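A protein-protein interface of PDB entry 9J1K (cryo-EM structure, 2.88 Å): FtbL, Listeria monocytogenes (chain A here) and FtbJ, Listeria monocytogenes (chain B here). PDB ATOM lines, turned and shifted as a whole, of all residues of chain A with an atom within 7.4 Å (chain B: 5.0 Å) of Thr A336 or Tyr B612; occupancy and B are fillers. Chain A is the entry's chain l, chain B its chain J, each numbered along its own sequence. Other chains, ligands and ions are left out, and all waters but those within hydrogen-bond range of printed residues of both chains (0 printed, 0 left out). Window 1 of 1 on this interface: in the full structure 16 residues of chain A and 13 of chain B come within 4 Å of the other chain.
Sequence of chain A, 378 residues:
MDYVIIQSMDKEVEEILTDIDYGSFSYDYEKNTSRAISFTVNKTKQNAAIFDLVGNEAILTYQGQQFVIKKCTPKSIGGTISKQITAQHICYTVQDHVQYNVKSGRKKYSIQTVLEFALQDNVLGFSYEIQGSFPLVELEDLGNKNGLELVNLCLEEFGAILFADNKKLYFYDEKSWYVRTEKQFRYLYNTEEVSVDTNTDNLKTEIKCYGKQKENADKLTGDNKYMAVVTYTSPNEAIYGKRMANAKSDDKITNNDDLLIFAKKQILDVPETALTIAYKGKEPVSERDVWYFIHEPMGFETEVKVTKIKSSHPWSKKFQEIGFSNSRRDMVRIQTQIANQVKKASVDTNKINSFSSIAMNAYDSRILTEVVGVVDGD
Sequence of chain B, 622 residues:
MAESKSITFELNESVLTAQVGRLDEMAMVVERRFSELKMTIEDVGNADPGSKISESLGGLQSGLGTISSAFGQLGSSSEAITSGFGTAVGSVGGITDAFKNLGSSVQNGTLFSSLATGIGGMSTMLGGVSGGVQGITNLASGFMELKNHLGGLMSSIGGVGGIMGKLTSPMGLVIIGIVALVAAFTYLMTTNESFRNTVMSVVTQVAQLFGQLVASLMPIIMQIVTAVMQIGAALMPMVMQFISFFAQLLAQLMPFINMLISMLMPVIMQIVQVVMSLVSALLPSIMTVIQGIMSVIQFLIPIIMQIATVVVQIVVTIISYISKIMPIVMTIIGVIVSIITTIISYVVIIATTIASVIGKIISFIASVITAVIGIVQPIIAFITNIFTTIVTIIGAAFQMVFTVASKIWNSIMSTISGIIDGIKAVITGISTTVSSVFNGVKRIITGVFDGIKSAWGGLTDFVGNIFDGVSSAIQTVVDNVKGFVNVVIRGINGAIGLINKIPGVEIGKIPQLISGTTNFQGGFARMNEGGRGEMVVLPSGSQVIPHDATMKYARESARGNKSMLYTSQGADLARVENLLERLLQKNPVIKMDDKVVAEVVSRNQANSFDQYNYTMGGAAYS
The side-chain hydroxyl (OG1) of Thr B615 lies close to the backbone carbonyl oxygen (O) of Thr A33, 3.4 Å away.
NE2 of Gln A335 lies close to SD of Met A331.
The backbone NH (N) of Val A332 lies within hydrogen-bond range of the side-chain carboxylate (OD1) of Asp A330 (3.3 Å).
O of Thr A336 sits at hydrogen-bond distance from ND2 of Asn A340 (3.3 Å).
The side-chain hydroxyl of Ser A327 is in hydrogen-bond range of the guanidinium group of Arg A333, at 3.2 Å.
O of Gln A337 lies close to OD1 of Asn A340 (2.7 Å).
O of Val A332 lies within hydrogen-bond range of OG1 of Thr A336, at 3.1 Å.
Among the printed residues, merely in contact across the chains: Thr A33 with Tyr B612 (3.9 Å), Gln A88 with Gln B611 (3.2 Å), Gln A88 with Tyr B614 (3.9 Å), Gln A88 with Thr B615 (3.6 Å), Asn A152 with Thr B615 (3.8 Å), Asn A152 with Met B616 (3.6 Å), Val A332 with Tyr B612 (3.5 Å), Arg A333 with Tyr B612 (3.5 Å), Gln A335 with Phe B609 (3.9 Å), Thr A336 with Phe B609 (3.6 Å), Thr A336 with Tyr B612 (3.9 Å) and Asn A340 with Ala B619 (3.4 Å).
Printed residues of chain B within 4 Å of Asn A152: Thr B615 (3.8 Å) and Met B616 (3.6 Å).
Thr A336 touches just these residues of chain B: Phe B609 and Tyr B612.
Ile A338 touches none of the printed residues of chain B.
Of the printed residues of chain A, Gln B611 touches Gln A88.
Of chain A, only Thr A33 (3.9 Å), Val A332 (3.5 Å), Arg A333 (3.5 Å) and Thr A336 (3.9 Å) come within 4 Å of Tyr B612.
Of the printed residues of chain A, Tyr B614 touches Gln A88.
Printed residues of chain A within 4 Å of Thr B615: Thr A33, Gln A88 and Asn A152.
Of the 10 printed residues of chain B, 7 touch a printed residue of chain A.
Printed residues of chain B that touch a printed residue of chain A: Phe B609, Gln B611, Tyr B612, Tyr B614, Thr B615, Met B616 and Ala B619.
Hydrophobic or aromatic side chains of chain B within 4 Å of the printed part of chain A: Phe B609, Tyr B612 and Tyr B614.
Hydrophobic or aromatic side chains of chain A within 4 Å of the printed part of chain B: Val A332.
Among the printed residues, 13 pairs touch across the chains.
Among the printed residues, no Asp or Glu carboxylate lies within 4 Å of a Lys or Arg side-chain nitrogen of the other chain.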
ATOM      1  N   ASP A  28      11.935 -24.263  -4.778  1.00  0.00           N
ATOM      2  CA  ASP A  28      10.713 -25.033  -4.952  1.00  0.00           C
ATOM      3  C   ASP A  28       9.581 -24.113  -5.381  1.00  0.00           C
ATOM      4  O   ASP A  28       9.338 -23.079  -4.748  1.00  0.00           O
ATOM      5  CB  ASP A  28      10.339 -25.762  -3.660  1.00  0.00           C
ATOM      6  CG  ASP A  28      11.118 -27.047  -3.472  1.00  0.00           C
ATOM      7  OD1 ASP A  28      12.345 -27.038  -3.708  1.00  0.00           O
ATOM      8  OD2 ASP A  28      10.507 -28.065  -3.088  1.00  0.00           O
ATOM      9  N   GLU A  30       5.392 -24.348  -6.935  1.00  0.00           N
ATOM     10  CA  GLU A  30       4.204 -25.099  -7.315  1.00  0.00           C
ATOM     11  C   GLU A  30       3.071 -24.105  -7.500  1.00  0.00           C
ATOM     12  O   GLU A  30       2.825 -23.278  -6.614  1.00  0.00           O
ATOM     13  CB  GLU A  30       3.840 -26.150  -6.264  1.00  0.00           C
ATOM     14  CG  GLU A  30       2.738 -27.097  -6.704  1.00  0.00           C
ATOM     15  CD  GLU A  30       2.326 -28.061  -5.611  1.00  0.00           C
ATOM     16  OE1 GLU A  30       3.068 -28.183  -4.615  1.00  0.00           O
ATOM     17  OE2 GLU A  30       1.262 -28.697  -5.749  1.00  0.00           O
ATOM     18  N   THR A  33       0.508 -22.757  -5.063  1.00  0.00           N
ATOM     19  CA  THR A  33       0.801 -23.515  -3.855  1.00  0.00           C
ATOM     20  C   THR A  33       1.998 -22.978  -3.089  1.00  0.00           C
ATOM     21  O   THR A  33       1.872 -22.680  -1.896  1.00  0.00           O
ATOM     22  CB  THR A  33       1.027 -24.994  -4.202  1.00  0.00           C
ATOM     23  OG1 THR A  33      -0.184 -25.552  -4.726  1.00  0.00           O
ATOM     24  CG2 THR A  33       1.440 -25.772  -2.965  1.00  0.00           C
ATOM     25  N   SER A  34       3.159 -22.840  -3.727  1.00  0.00           N
ATOM     26  CA  SER A  34       4.342 -22.460  -2.966  1.00  0.00           C
ATOM     27  C   SER A  34       5.395 -21.859  -3.883  1.00  0.00           C
ATOM     28  O   SER A  34       5.437 -22.138  -5.082  1.00  0.00           O
ATOM     29  CB  SER A  34       4.925 -23.659  -2.210  1.00  0.00           C
ATOM     30  OG  SER A  34       4.865 -24.833  -3.000  1.00  0.00           O
ATOM     31  N   GLN A  88      10.413 -17.646   1.913  1.00  0.00           N
ATOM     32  CA  GLN A  88       9.256 -17.687   1.033  1.00  0.00           C
ATOM     33  C   GLN A  88       9.190 -16.414   0.203  1.00  0.00           C
ATOM     34  O   GLN A  88       9.666 -15.360   0.625  1.00  0.00           O
ATOM     35  CB  GLN A  88       7.964 -17.847   1.833  1.00  0.00           C
ATOM     36  CG  GLN A  88       8.101 -18.743   3.043  1.00  0.00           C
ATOM     37  CD  GLN A  88       7.776 -20.185   2.732  1.00  0.00           C
ATOM     38  OE1 GLN A  88       7.027 -20.479   1.801  1.00  0.00           O
ATOM     39  NE2 GLN A  88       8.342 -21.096   3.509  1.00  0.00           N
ATOM     40  N   ASN A 152      -6.159 -16.495  -2.215  1.00  0.00           N
ATOM     41  CA  ASN A 152      -6.407 -17.917  -2.415  1.00  0.00           C
ATOM     42  C   ASN A 152      -7.861 -18.173  -2.786  1.00  0.00           C
ATOM     43  O   ASN A 152      -8.156 -19.049  -3.606  1.00  0.00           O
ATOM     44  CB  ASN A 152      -6.027 -18.699  -1.159  1.00  0.00           C
ATOM     45  CG  ASN A 152      -4.528 -18.817  -0.979  1.00  0.00           C
ATOM     46  OD1 ASN A 152      -3.760 -18.573  -1.908  1.00  0.00           O
ATOM     47  ND2 ASN A 152      -4.104 -19.194   0.221  1.00  0.00           N
ATOM     48  N   LYS A 308       4.901 -27.950 -11.329  1.00  0.00           N
ATOM     49  CA  LYS A 308       5.735 -27.995 -10.137  1.00  0.00           C
ATOM     50  C   LYS A 308       7.189 -28.149 -10.554  1.00  0.00           C
ATOM     51  O   LYS A 308       7.508 -28.957 -11.429  1.00  0.00           O
ATOM     52  CB  LYS A 308       5.320 -29.143  -9.210  1.00  0.00           C
ATOM     53  CG  LYS A 308       6.381 -29.546  -8.204  1.00  0.00           C
ATOM     54  CD  LYS A 308       6.002 -30.830  -7.489  1.00  0.00           C
ATOM     55  CE  LYS A 308       4.749 -30.643  -6.654  1.00  0.00           C
ATOM     56  NZ  LYS A 308       4.911 -31.192  -5.282  1.00  0.00           N
ATOM     57  N   SER A 327      -0.077 -33.067  -8.261  1.00  0.00           N
ATOM     58  CA  SER A 327       1.043 -33.643  -7.531  1.00  0.00           C
ATOM     59  C   SER A 327       0.641 -34.948  -6.855  1.00  0.00           C
ATOM     60  O   SER A 327      -0.538 -35.293  -6.752  1.00  0.00           O
ATOM     61  CB  SER A 327       1.577 -32.655  -6.487  1.00  0.00           C
ATOM     62  OG  SER A 327       0.574 -32.325  -5.543  1.00  0.00           O
ATOM     63  N   ASP A 330       0.864 -37.631  -0.822  1.00  0.00           N
ATOM     64  CA  ASP A 330       1.574 -37.108   0.345  1.00  0.00           C
ATOM     65  C   ASP A 330       0.649 -36.971   1.554  1.00  0.00           C
ATOM     66  O   ASP A 330      -0.566 -36.808   1.407  1.00  0.00           O
ATOM     67  CB  ASP A 330       2.238 -35.770   0.005  1.00  0.00           C
ATOM     68  CG  ASP A 330       3.205 -35.302   1.075  1.00  0.00           C
ATOM     69  OD1 ASP A 330       3.335 -35.981   2.113  1.00  0.00           O
ATOM     70  OD2 ASP A 330       3.849 -34.253   0.867  1.00  0.00           O
ATOM     71  N   MET A 331       1.213 -37.045   2.761  1.00  0.00           N
ATOM     72  CA  MET A 331       0.406 -36.935   3.971  1.00  0.00           C
ATOM     73  C   MET A 331       0.231 -35.507   4.466  1.00  0.00           C
ATOM     74  O   MET A 331      -0.861 -35.152   4.917  1.00  0.00           O
ATOM     75  CB  MET A 331       0.992 -37.793   5.095  1.00  0.00           C
ATOM     76  CG  MET A 331       0.204 -37.681   6.398  1.00  0.00           C
ATOM     77  SD  MET A 331      -1.154 -38.832   6.670  1.00  0.00           S
ATOM     78  CE  MET A 331      -0.686 -40.179   5.610  1.00  0.00           C
ATOM     79  N   VAL A 332       1.275 -34.677   4.397  1.00  0.00           N
ATOM     80  CA  VAL A 332       1.168 -33.328   4.944  1.00  0.00           C
ATOM     81  C   VAL A 332       0.054 -32.551   4.254  1.00  0.00           C
ATOM     82  O   VAL A 332      -0.624 -31.731   4.885  1.00  0.00           O
ATOM     83  CB  VAL A 332       2.523 -32.601   4.848  1.00  0.00           C
ATOM     84  CG1 VAL A 332       3.560 -33.315   5.698  1.00  0.00           C
ATOM     85  CG2 VAL A 332       2.987 -32.522   3.407  1.00  0.00           C
ATOM     86  N   ARG A 333      -0.179 -32.813   2.965  1.00  0.00           N
ATOM     87  CA  ARG A 333      -1.315 -32.203   2.284  1.00  0.00           C
ATOM     88  C   ARG A 333      -2.631 -32.650   2.909  1.00  0.00           C
ATOM     89  O   ARG A 333      -3.540 -31.835   3.114  1.00  0.00           O
ATOM     90  CB  ARG A 333      -1.284 -32.554   0.797  1.00  0.00           C
ATOM     91  CG  ARG A 333       0.097 -32.907   0.273  1.00  0.00           C
ATOM     92  CD  ARG A 333       0.928 -31.670  -0.009  1.00  0.00           C
ATOM     93  NE  ARG A 333       0.158 -30.634  -0.686  1.00  0.00           N
ATOM     94  CZ  ARG A 333       0.286 -30.327  -1.969  1.00  0.00           C
ATOM     95  NH1 ARG A 333       1.145 -30.962  -2.749  1.00  0.00           N
ATOM     96  NH2 ARG A 333      -0.468 -29.359  -2.483  1.00  0.00           N
ATOM     97  N   ILE A 334      -2.746 -33.942   3.222  1.00  0.00           N
ATOM     98  CA  ILE A 334      -3.961 -34.456   3.850  1.00  0.00           C
ATOM     99  C   ILE A 334      -4.164 -33.816   5.217  1.00  0.00           C
ATOM    100  O   ILE A 334      -5.288 -33.462   5.594  1.00  0.00           O
ATOM    101  CB  ILE A 334      -3.898 -35.991   3.946  1.00  0.00           C
ATOM    102  CG1 ILE A 334      -3.775 -36.607   2.554  1.00  0.00           C
ATOM    103  CG2 ILE A 334      -5.126 -36.533   4.656  1.00  0.00           C
ATOM    104  CD1 ILE A 334      -3.473 -38.086   2.570  1.00  0.00           C
ATOM    105  N   GLN A 335      -3.082 -33.669   5.984  1.00  0.00           N
ATOM    106  CA  GLN A 335      -3.184 -33.035   7.293  1.00  0.00           C
ATOM    107  C   GLN A 335      -3.612 -31.580   7.172  1.00  0.00           C
ATOM    108  O   GLN A 335      -4.419 -31.098   7.973  1.00  0.00           O
ATOM    109  CB  GLN A 335      -1.856 -33.148   8.042  1.00  0.00           C
ATOM    110  CG  GLN A 335      -1.222 -34.525   7.973  1.00  0.00           C
ATOM    111  CD  GLN A 335      -1.843 -35.508   8.947  1.00  0.00           C
ATOM    112  OE1 GLN A 335      -2.920 -35.268   9.493  1.00  0.00           O
ATOM    113  NE2 GLN A 335      -1.168 -36.629   9.163  1.00  0.00           N
ATOM    114  N   THR A 336      -3.081 -30.861   6.181  1.00  0.00           N
ATOM    115  CA  THR A 336      -3.508 -29.480   5.971  1.00  0.00           C
ATOM    116  C   THR A 336      -4.984 -29.409   5.601  1.00  0.00           C
ATOM    117  O   THR A 336      -5.711 -28.529   6.082  1.00  0.00           O
ATOM    118  CB  THR A 336      -2.657 -28.818   4.889  1.00  0.00           C
ATOM    119  OG1 THR A 336      -2.647 -29.639   3.715  1.00  0.00           O
ATOM    120  CG2 THR A 336      -1.232 -28.614   5.377  1.00  0.00           C
ATOM    121  N   GLN A 337      -5.445 -30.321   4.743  1.00  0.00           N
ATOM    122  CA  GLN A 337      -6.861 -30.347   4.383  1.00  0.00           C
ATOM    123  C   GLN A 337      -7.728 -30.615   5.607  1.00  0.00           C
ATOM    124  O   GLN A 337      -8.754 -29.954   5.816  1.00  0.00           O
ATOM    125  CB  GLN A 337      -7.114 -31.400   3.304  1.00  0.00           C
ATOM    126  CG  GLN A 337      -6.373 -31.155   2.002  1.00  0.00           C
ATOM    127  CD  GLN A 337      -6.599 -29.761   1.457  1.00  0.00           C
ATOM    128  OE1 GLN A 337      -5.775 -28.866   1.646  1.00  0.00           O
ATOM    129  NE2 GLN A 337      -7.722 -29.566   0.776  1.00  0.00           N
ATOM    130  N   ILE A 338      -7.324 -31.579   6.434  1.00  0.00           N
ATOM    131  CA  ILE A 338      -8.087 -31.893   7.638  1.00  0.00           C
ATOM    132  C   ILE A 338      -8.108 -30.698   8.581  1.00  0.00           C
ATOM    133  O   ILE A 338      -9.141 -30.376   9.176  1.00  0.00           O
ATOM    134  CB  ILE A 338      -7.516 -33.150   8.320  1.00  0.00           C
ATOM    135  CG1 ILE A 338      -7.783 -34.386   7.460  1.00  0.00           C
ATOM    136  CG2 ILE A 338      -8.116 -33.329   9.704  1.00  0.00           C
ATOM    137  CD1 ILE A 338      -7.359 -35.684   8.107  1.00  0.00           C
ATOM    138  N   ALA A 339      -6.969 -30.015   8.724  1.00  0.00           N
ATOM    139  CA  ALA A 339      -6.901 -28.862   9.615  1.00  0.00           C
ATOM    140  C   ALA A 339      -7.798 -27.728   9.135  1.00  0.00           C
ATOM    141  O   ALA A 339      -8.491 -27.092   9.939  1.00  0.00           O
ATOM    142  CB  ALA A 339      -5.456 -28.385   9.744  1.00  0.00           C
ATOM    143  N   ASN A 340      -7.799 -27.449   7.828  1.00  0.00           N
ATOM    144  CA  ASN A 340      -8.640 -26.363   7.336  1.00  0.00           C
ATOM    145  C   ASN A 340     -10.118 -26.727   7.436  1.00  0.00           C
ATOM    146  O   ASN A 340     -10.955 -25.866   7.732  1.00  0.00           O
ATOM    147  CB  ASN A 340      -8.235 -25.968   5.909  1.00  0.00           C
ATOM    148  CG  ASN A 340      -8.610 -27.002   4.851  1.00  0.00           C
ATOM    149  OD1 ASN A 340      -9.680 -27.608   4.884  1.00  0.00           O
ATOM    150  ND2 ASN A 340      -7.715 -27.194   3.891  1.00  0.00           N
ATOM    151  N   GLN A 341     -10.456 -28.001   7.214  1.00  0.00           N
ATOM    152  CA  GLN A 341     -11.833 -28.436   7.427  1.00  0.00           C
ATOM    153  C   GLN A 341     -12.233 -28.288   8.889  1.00  0.00           C
ATOM    154  O   GLN A 341     -13.363 -27.895   9.198  1.00  0.00           O
ATOM    155  CB  GLN A 341     -12.006 -29.882   6.965  1.00  0.00           C
ATOM    156  CG  GLN A 341     -12.495 -30.019   5.534  1.00  0.00           C
ATOM    157  CD  GLN A 341     -12.299 -31.418   4.984  1.00  0.00           C
ATOM    158  OE1 GLN A 341     -12.544 -32.408   5.673  1.00  0.00           O
ATOM    159  NE2 GLN A 341     -11.854 -31.506   3.736  1.00  0.00           N
ATOM    160  N   VAL A 342     -11.313 -28.600   9.805  1.00  0.00           N
ATOM    161  CA  VAL A 342     -11.582 -28.440  11.230  1.00  0.00           C
ATOM    162  C   VAL A 342     -11.829 -26.976  11.563  1.00  0.00           C
ATOM    163  O   VAL A 342     -12.744 -26.643  12.323  1.00  0.00           O
ATOM    164  CB  VAL A 342     -10.420 -29.020  12.059  1.00  0.00           C
ATOM    165  CG1 VAL A 342     -10.396 -28.414  13.453  1.00  0.00           C
ATOM    166  CG2 VAL A 342     -10.524 -30.528  12.129  1.00  0.00           C
ATOM    167  N   SER B 608       7.420 -29.153   6.905  1.00  0.00           N
ATOM    168  CA  SER B 608       6.630 -29.105   5.677  1.00  0.00           C
ATOM    169  C   SER B 608       5.215 -28.604   5.947  1.00  0.00           C
ATOM    170  O   SER B 608       4.664 -27.813   5.169  1.00  0.00           O
ATOM    171  CB  SER B 608       6.595 -30.484   5.020  1.00  0.00           C
ATOM    172  OG  SER B 608       7.898 -30.914   4.672  1.00  0.00           O
ATOM    173  N   PHE B 609       4.608 -29.063   7.043  1.00  0.00           N
ATOM    174  CA  PHE B 609       3.260 -28.630   7.394  1.00  0.00           C
ATOM    175  C   PHE B 609       3.218 -27.137   7.681  1.00  0.00           C
ATOM    176  O   PHE B 609       2.285 -26.445   7.264  1.00  0.00           O
ATOM    177  CB  PHE B 609       2.758 -29.426   8.600  1.00  0.00           C
ATOM    178  CG  PHE B 609       1.390 -29.022   9.070  1.00  0.00           C
ATOM    179  CD1 PHE B 609       0.257 -29.591   8.514  1.00  0.00           C
ATOM    180  CD2 PHE B 609       1.234 -28.085  10.078  1.00  0.00           C
ATOM    181  CE1 PHE B 609      -1.001 -29.226   8.946  1.00  0.00           C
ATOM    182  CE2 PHE B 609      -0.022 -27.716  10.512  1.00  0.00           C
ATOM    183  CZ  PHE B 609      -1.141 -28.288   9.947  1.00  0.00           C
ATOM    184  N   ASP B 610       4.216 -26.626   8.405  1.00  0.00           N
ATOM    185  CA  ASP B 610       4.277 -25.195   8.677  1.00  0.00           C
ATOM    186  C   ASP B 610       4.450 -24.402   7.390  1.00  0.00           C
ATOM    187  O   ASP B 610       3.833 -23.344   7.218  1.00  0.00           O
ATOM    188  CB  ASP B 610       5.414 -24.893   9.651  1.00  0.00           C
ATOM    189  CG  ASP B 610       5.077 -25.279  11.075  1.00  0.00           C
ATOM    190  OD1 ASP B 610       3.875 -25.406  11.388  1.00  0.00           O
ATOM    191  OD2 ASP B 610       6.013 -25.452  11.882  1.00  0.00           O
ATOM    192  N   GLN B 611       5.287 -24.897   6.477  1.00  0.00           N
ATOM    193  CA  GLN B 611       5.449 -24.234   5.186  1.00  0.00           C
ATOM    194  C   GLN B 611       4.123 -24.162   4.439  1.00  0.00           C
ATOM    195  O   GLN B 611       3.734 -23.102   3.929  1.00  0.00           O
ATOM    196  CB  GLN B 611       6.493 -24.977   4.353  1.00  0.00           C
ATOM    197  CG  GLN B 611       7.783 -24.218   4.141  1.00  0.00           C
ATOM    198  CD  GLN B 611       8.594 -24.773   2.991  1.00  0.00           C
ATOM    199  OE1 GLN B 611       8.134 -24.807   1.850  1.00  0.00           O
ATOM    200  NE2 GLN B 611       9.811 -25.215   3.285  1.00  0.00           N
ATOM    201  N   TYR B 612       3.408 -25.288   4.376  1.00  0.00           N
ATOM    202  CA  TYR B 612       2.145 -25.324   3.647  1.00  0.00           C
ATOM    203  C   TYR B 612       1.103 -24.426   4.302  1.00  0.00           C
ATOM    204  O   TYR B 612       0.327 -23.756   3.610  1.00  0.00           O
ATOM    205  CB  TYR B 612       1.641 -26.761   3.552  1.00  0.00           C
ATOM    206  CG  TYR B 612       2.262 -27.530   2.412  1.00  0.00           C
ATOM    207  CD1 TYR B 612       2.649 -28.852   2.569  1.00  0.00           C
ATOM    208  CD2 TYR B 612       2.469 -26.929   1.178  1.00  0.00           C
ATOM    209  CE1 TYR B 612       3.223 -29.555   1.530  1.00  0.00           C
ATOM    210  CE2 TYR B 612       3.040 -27.625   0.133  1.00  0.00           C
ATOM    211  CZ  TYR B 612       3.415 -28.938   0.314  1.00  0.00           C
ATOM    212  OH  TYR B 612       3.984 -29.636  -0.724  1.00  0.00           O
ATOM    213  N   ASN B 613       1.065 -24.404   5.636  1.00  0.00           N
ATOM    214  CA  ASN B 613       0.142 -23.518   6.338  1.00  0.00           C
ATOM    215  C   ASN B 613       0.463 -22.057   6.053  1.00  0.00           C
ATOM    216  O   ASN B 613      -0.444 -21.248   5.826  1.00  0.00           O
ATOM    217  CB  ASN B 613       0.191 -23.801   7.839  1.00  0.00           C
ATOM    218  CG  ASN B 613      -0.498 -22.729   8.663  1.00  0.00           C
ATOM    219  OD1 ASN B 613      -1.498 -22.147   8.244  1.00  0.00           O
ATOM    220  ND2 ASN B 613       0.039 -22.463   9.848  1.00  0.00           N
ATOM    221  N   TYR B 614       1.749 -21.699   6.060  1.00  0.00           N
ATOM    222  CA  TYR B 614       2.126 -20.318   5.779  1.00  0.00           C
ATOM    223  C   TYR B 614       1.739 -19.923   4.361  1.00  0.00           C
ATOM    224  O   TYR B 614       1.258 -18.809   4.129  1.00  0.00           O
ATOM    225  CB  TYR B 614       3.625 -20.122   5.996  1.00  0.00           C
ATOM    226  CG  TYR B 614       4.076 -18.693   5.811  1.00  0.00           C
ATOM    227  CD1 TYR B 614       4.034 -17.791   6.864  1.00  0.00           C
ATOM    228  CD2 TYR B 614       4.534 -18.241   4.581  1.00  0.00           C
ATOM    229  CE1 TYR B 614       4.442 -16.484   6.702  1.00  0.00           C
ATOM    230  CE2 TYR B 614       4.942 -16.935   4.408  1.00  0.00           C
ATOM    231  CZ  TYR B 614       4.894 -16.061   5.472  1.00  0.00           C
ATOM    232  OH  TYR B 614       5.299 -14.758   5.304  1.00  0.00           O
ATOM    233  N   THR B 615       1.943 -20.822   3.396  1.00  0.00           N
ATOM    234  CA  THR B 615       1.550 -20.518   2.026  1.00  0.00           C
ATOM    235  C   THR B 615       0.037 -20.435   1.863  1.00  0.00           C
ATOM    236  O   THR B 615      -0.435 -19.904   0.854  1.00  0.00           O
ATOM    237  CB  THR B 615       2.114 -21.564   1.065  1.00  0.00           C
ATOM    238  OG1 THR B 615       1.714 -22.873   1.490  1.00  0.00           O
ATOM    239  CG2 THR B 615       3.631 -21.488   1.027  1.00  0.00           C
ATOM    240  N   MET B 616      -0.727 -20.946   2.829  1.00  0.00           N
ATOM    241  CA  MET B 616      -2.183 -20.876   2.810  1.00  0.00           C
ATOM    242  C   MET B 616      -2.720 -19.816   3.763  1.00  0.00           C
ATOM    243  O   MET B 616      -3.858 -19.921   4.232  1.00  0.00           O
ATOM    244  CB  MET B 616      -2.782 -22.240   3.149  1.00  0.00           C
ATOM    245  CG  MET B 616      -2.975 -23.154   1.952  1.00  0.00           C
ATOM    246  SD  MET B 616      -3.719 -24.739   2.385  1.00  0.00           S
ATOM    247  CE  MET B 616      -3.425 -24.796   4.150  1.00  0.00           C
ATOM    248  N   ALA B 619      -5.172 -20.589   7.316  1.00  0.00           N
ATOM    249  CA  ALA B 619      -6.284 -21.539   7.272  1.00  0.00           C
ATOM    250  C   ALA B 619      -5.762 -22.951   7.537  1.00  0.00           C
ATOM    251  O   ALA B 619      -5.766 -23.834   6.676  1.00  0.00           O
ATOM    252  CB  ALA B 619      -7.009 -21.447   5.937  1.00  0.00           C
